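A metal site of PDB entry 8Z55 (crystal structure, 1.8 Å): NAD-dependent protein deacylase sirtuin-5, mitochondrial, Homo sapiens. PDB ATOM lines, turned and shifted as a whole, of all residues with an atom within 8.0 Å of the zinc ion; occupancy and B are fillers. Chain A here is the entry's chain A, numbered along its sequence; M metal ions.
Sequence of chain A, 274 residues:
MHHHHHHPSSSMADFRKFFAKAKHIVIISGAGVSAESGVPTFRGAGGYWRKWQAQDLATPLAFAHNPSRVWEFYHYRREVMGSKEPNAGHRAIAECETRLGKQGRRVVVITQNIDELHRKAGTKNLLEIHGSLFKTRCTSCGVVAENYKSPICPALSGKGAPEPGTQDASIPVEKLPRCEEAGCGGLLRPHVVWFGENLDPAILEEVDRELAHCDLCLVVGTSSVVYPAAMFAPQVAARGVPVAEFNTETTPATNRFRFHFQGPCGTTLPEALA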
ATOM      1  N   ARG A 137      24.809  -7.920  -6.397  1.00  0.00           N
ATOM      2  CA  ARG A 137      24.438  -9.327  -6.325  1.00  0.00           C
ATOM      3  C   ARG A 137      25.672 -10.189  -6.514  1.00  0.00           C
ATOM      4  O   ARG A 137      26.472  -9.957  -7.439  1.00  0.00           O
ATOM      5  CB  ARG A 137      23.370  -9.701  -7.388  1.00  0.00           C
ATOM      6  CG  ARG A 137      22.974 -11.161  -7.296  1.00  0.00           C
ATOM      7  CD  ARG A 137      21.660 -11.456  -7.975  1.00  0.00           C
ATOM      8  NE  ARG A 137      21.804 -11.729  -9.401  1.00  0.00           N
ATOM      9  CZ  ARG A 137      21.450 -10.881 -10.362  1.00  0.00           C
ATOM     10  NH1 ARG A 137      20.936  -9.708 -10.053  1.00  0.00           N
ATOM     11  NH2 ARG A 137      21.604 -11.218 -11.638  1.00  0.00           N
ATOM     12  N   CYS A 138      25.831 -11.170  -5.652  1.00  0.00           N
ATOM     13  CA  CYS A 138      27.001 -12.044  -5.736  1.00  0.00           C
ATOM     14  C   CYS A 138      26.781 -13.099  -6.803  1.00  0.00           C
ATOM     15  O   CYS A 138      25.777 -13.818  -6.796  1.00  0.00           O
ATOM     16  CB  CYS A 138      27.259 -12.711  -4.392  1.00  0.00           C
ATOM     17  SG  CYS A 138      28.684 -13.772  -4.490  1.00  0.00           S
ATOM     18  N   THR A 139      27.736 -13.194  -7.734  1.00  0.00           N
ATOM     19  CA  THR A 139      27.639 -14.184  -8.797  1.00  0.00           C
ATOM     20  C   THR A 139      27.812 -15.620  -8.306  1.00  0.00           C
ATOM     21  O   THR A 139      27.555 -16.550  -9.075  1.00  0.00           O
ATOM     22  CB  THR A 139      28.630 -13.875  -9.931  1.00  0.00           C
ATOM     23  OG1 THR A 139      29.972 -13.897  -9.432  1.00  0.00           O
ATOM     24  CG2 THR A 139      28.346 -12.512 -10.551  1.00  0.00           C
ATOM     25  N   SER A 140      28.247 -15.824  -7.056  1.00  0.00           N
ATOM     26  CA  SER A 140      28.408 -17.170  -6.512  1.00  0.00           C
ATOM     27  C   SER A 140      27.219 -17.591  -5.648  1.00  0.00           C
ATOM     28  O   SER A 140      26.549 -18.577  -5.959  1.00  0.00           O
ATOM     29  CB  SER A 140      29.705 -17.278  -5.697  1.00  0.00           C
ATOM     30  OG  SER A 140      30.833 -17.195  -6.534  1.00  0.00           O
ATOM     31  N   CYS A 141      26.939 -16.846  -4.591  1.00  0.00           N
ATOM     32  CA  CYS A 141      25.863 -17.229  -3.684  1.00  0.00           C
ATOM     33  C   CYS A 141      24.537 -16.539  -4.004  1.00  0.00           C
ATOM     34  O   CYS A 141      23.492 -17.000  -3.531  1.00  0.00           O
ATOM     35  CB  CYS A 141      26.261 -16.959  -2.220  1.00  0.00           C
ATOM     36  SG  CYS A 141      26.469 -15.223  -1.787  1.00  0.00           S
ATOM     37  N   GLY A 142      24.553 -15.484  -4.814  1.00  0.00           N
ATOM     38  CA  GLY A 142      23.327 -14.801  -5.213  1.00  0.00           C
ATOM     39  C   GLY A 142      22.799 -13.776  -4.233  1.00  0.00           C
ATOM     40  O   GLY A 142      21.743 -13.186  -4.509  1.00  0.00           O
ATOM     41  N   VAL A 143      23.482 -13.525  -3.120  1.00  0.00           N
ATOM     42  CA  VAL A 143      22.975 -12.595  -2.121  1.00  0.00           C
ATOM     43  C   VAL A 143      22.956 -11.173  -2.680  1.00  0.00           C
ATOM     44  O   VAL A 143      23.890 -10.737  -3.357  1.00  0.00           O
ATOM     45  CB  VAL A 143      23.822 -12.690  -0.835  1.00  0.00           C
ATOM     46  CG1 VAL A 143      23.648 -11.445   0.019  1.00  0.00           C
ATOM     47  CG2 VAL A 143      23.448 -13.939  -0.058  1.00  0.00           C
ATOM     48  N   VAL A 144      21.859 -10.452  -2.422  1.00  0.00           N
ATOM     49  CA  VAL A 144      21.712  -9.051  -2.849  1.00  0.00           C
ATOM     50  C   VAL A 144      21.911  -8.143  -1.639  1.00  0.00           C
ATOM     51  O   VAL A 144      21.465  -8.456  -0.521  1.00  0.00           O
ATOM     52  CB  VAL A 144      20.367  -8.824  -3.550  1.00  0.00           C
ATOM     53  CG1 VAL A 144      20.197  -9.853  -4.637  1.00  0.00           C
ATOM     54  CG2 VAL A 144      19.231  -8.931  -2.557  1.00  0.00           C
ATOM     55  N   ARG A 178      33.908  -7.747  -4.077  1.00  0.00           N
ATOM     56  CA  ARG A 178      33.793  -9.146  -3.691  1.00  0.00           C
ATOM     57  C   ARG A 178      32.723  -9.311  -2.619  1.00  0.00           C
ATOM     58  O   ARG A 178      32.514  -8.426  -1.781  1.00  0.00           O
ATOM     59  CB  ARG A 178      35.127  -9.681  -3.140  1.00  0.00           C
ATOM     60  CG  ARG A 178      36.297  -9.503  -4.074  1.00  0.00           C
ATOM     61  CD  ARG A 178      36.091 -10.161  -5.429  1.00  0.00           C
ATOM     62  NE  ARG A 178      35.940 -11.613  -5.364  1.00  0.00           N
ATOM     63  CZ  ARG A 178      36.104 -12.412  -6.421  1.00  0.00           C
ATOM     64  NH1 ARG A 178      36.435 -11.893  -7.600  1.00  0.00           N
ATOM     65  NH2 ARG A 178      35.934 -13.723  -6.310  1.00  0.00           N
ATOM     66  N   CYS A 179      32.069 -10.460  -2.643  1.00  0.00           N
ATOM     67  CA  CYS A 179      31.056 -10.786  -1.644  1.00  0.00           C
ATOM     68  C   CYS A 179      31.692 -10.881  -0.268  1.00  0.00           C
ATOM     69  O   CYS A 179      32.720 -11.549  -0.094  1.00  0.00           O
ATOM     70  CB  CYS A 179      30.422 -12.125  -2.002  1.00  0.00           C
ATOM     71  SG  CYS A 179      29.035 -12.600  -0.956  1.00  0.00           S
ATOM     72  N   GLU A 180      31.100 -10.193   0.713  1.00  0.00           N
ATOM     73  CA  GLU A 180      31.566 -10.256   2.085  1.00  0.00           C
ATOM     74  C   GLU A 180      30.851 -11.317   2.920  1.00  0.00           C
ATOM     75  O   GLU A 180      31.134 -11.427   4.111  1.00  0.00           O
ATOM     76  CB  GLU A 180      31.468  -8.890   2.759  1.00  0.00           C
ATOM     77  CG  GLU A 180      32.632  -7.963   2.445  1.00  0.00           C
ATOM     78  CD  GLU A 180      32.404  -6.555   2.938  1.00  0.00           C
ATOM     79  OE1 GLU A 180      31.855  -5.736   2.166  1.00  0.00           O
ATOM     80  OE2 GLU A 180      32.766  -6.255   4.099  1.00  0.00           O
ATOM     81  N   GLU A 181      29.928 -12.070   2.326  1.00  0.00           N
ATOM     82  CA  GLU A 181      29.300 -13.170   3.049  1.00  0.00           C
ATOM     83  C   GLU A 181      30.378 -14.156   3.494  1.00  0.00           C
ATOM     84  O   GLU A 181      31.266 -14.520   2.706  1.00  0.00           O
ATOM     85  CB  GLU A 181      28.284 -13.871   2.152  1.00  0.00           C
ATOM     86  CG  GLU A 181      26.888 -14.008   2.748  1.00  0.00           C
ATOM     87  CD  GLU A 181      26.291 -12.678   3.190  1.00  0.00           C
ATOM     88  OE1 GLU A 181      25.473 -12.694   4.130  1.00  0.00           O
ATOM     89  OE2 GLU A 181      26.635 -11.634   2.602  1.00  0.00           O
ATOM     90  N   ALA A 182      30.298 -14.584   4.751  1.00  0.00           N
ATOM     91  CA  ALA A 182      31.302 -15.478   5.310  1.00  0.00           C
ATOM     92  C   ALA A 182      31.423 -16.732   4.461  1.00  0.00           C
ATOM     93  O   ALA A 182      30.450 -17.455   4.251  1.00  0.00           O
ATOM     94  CB  ALA A 182      30.917 -15.843   6.742  1.00  0.00           C
ATOM     95  N   GLY A 183      32.628 -16.987   3.968  1.00  0.00           N
ATOM     96  CA  GLY A 183      32.908 -18.161   3.182  1.00  0.00           C
ATOM     97  C   GLY A 183      32.651 -18.031   1.692  1.00  0.00           C
ATOM     98  O   GLY A 183      32.961 -18.967   0.942  1.00  0.00           O
ATOM     99  N   CYS A 184      32.101 -16.907   1.224  1.00  0.00           N
ATOM    100  CA  CYS A 184      31.881 -16.807  -0.211  1.00  0.00           C
ATOM    101  C   CYS A 184      33.030 -16.087  -0.918  1.00  0.00           C
ATOM    102  O   CYS A 184      33.843 -16.720  -1.595  1.00  0.00           O
ATOM    103  CB  CYS A 184      30.565 -16.088  -0.481  1.00  0.00           C
ATOM    104  SG  CYS A 184      30.184 -16.017  -2.208  1.00  0.00           S
ATOM    105  N   GLY A 185      33.166 -14.783  -0.676  1.00  0.00           N
ATOM    106  CA  GLY A 185      34.174 -14.006  -1.363  1.00  0.00           C
ATOM    107  C   GLY A 185      34.041 -13.951  -2.868  1.00  0.00           C
ATOM    108  O   GLY A 185      34.986 -13.541  -3.548  1.00  0.00           O
ATOM    109  N   GLY A 186      32.890 -14.327  -3.423  1.00  0.00           N
ATOM    110  CA  GLY A 186      32.720 -14.360  -4.865  1.00  0.00           C
ATOM    111  C   GLY A 186      32.650 -12.961  -5.482  1.00  0.00           C
ATOM    112  O   GLY A 186      32.647 -11.928  -4.804  1.00  0.00           O
ATOM    113  N   LEU A 187      32.617 -12.954  -6.809  1.00  0.00           N
ATOM    114  CA  LEU A 187      32.609 -11.706  -7.556  1.00  0.00           C
ATOM    115  C   LEU A 187      31.205 -11.120  -7.542  1.00  0.00           C
ATOM    116  O   LEU A 187      30.229 -11.810  -7.836  1.00  0.00           O
ATOM    117  CB  LEU A 187      33.047 -11.967  -8.997  1.00  0.00           C
ATOM    118  CG  LEU A 187      32.953 -10.758  -9.939  1.00  0.00           C
ATOM    119  CD1 LEU A 187      33.858  -9.610  -9.490  1.00  0.00           C
ATOM    120  CD2 LEU A 187      33.254 -11.136 -11.387  1.00  0.00           C
ATOM    121  N   LEU A 188      31.100  -9.842  -7.179  1.00  0.00           N
ATOM    122  CA  LEU A 188      29.816  -9.143  -7.236  1.00  0.00           C
ATOM    123  C   LEU A 188      29.606  -8.558  -8.626  1.00  0.00           C
ATOM    124  O   LEU A 188      30.556  -8.155  -9.294  1.00  0.00           O
ATOM    125  CB  LEU A 188      29.793  -7.989  -6.233  1.00  0.00           C
ATOM    126  CG  LEU A 188      29.986  -8.380  -4.773  1.00  0.00           C
ATOM    127  CD1 LEU A 188      29.945  -7.151  -3.865  1.00  0.00           C
ATOM    128  CD2 LEU A 188      28.905  -9.363  -4.394  1.00  0.00           C
HETATM  129 ZN    ZN M   1      28.582 -14.475  -2.279  1.00  0.00          ZN
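The side-chain sulfur of Cys 184 sits close to the backbone NH of Gly 186 (3.4 Å). The side-chain sulfur (SG) of Cys 141 sits close to the backbone NH (N) of Val 143, 3.7 Å away. The side-chain sulfur of Cys 138 lies close to the backbone NH of Ser 140. The backbone NH (N) of Cys 138 lies within hydrogen-bond range of the backbone carbonyl oxygen (O) of Val 143 (3.0 Å). O of Gly 186 sits at hydrogen-bond distance from N of Cys 179, 2.7 Å away. SG of Cys 179 lies close to N of Glu 181, at 3.4 Å. The backbone NH (N) of Gly 185 sits close to the backbone carbonyl oxygen (O) of Cys 179 (3.3 Å).
The zinc ion is bound by the side-chain sulfur (SG) of Cys 184 (2.2 Å), the side-chain sulfur (SG) of Cys 141 (2.3 Å), the side-chain sulfur (SG) of Cys 138 (2.3 Å) and the side-chain sulfur (SG) of Cys 179 (2.3 Å).
Within 4 Å of the zinc ion: Cys 138, Cys 141, Cys 179 and Cys 184.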
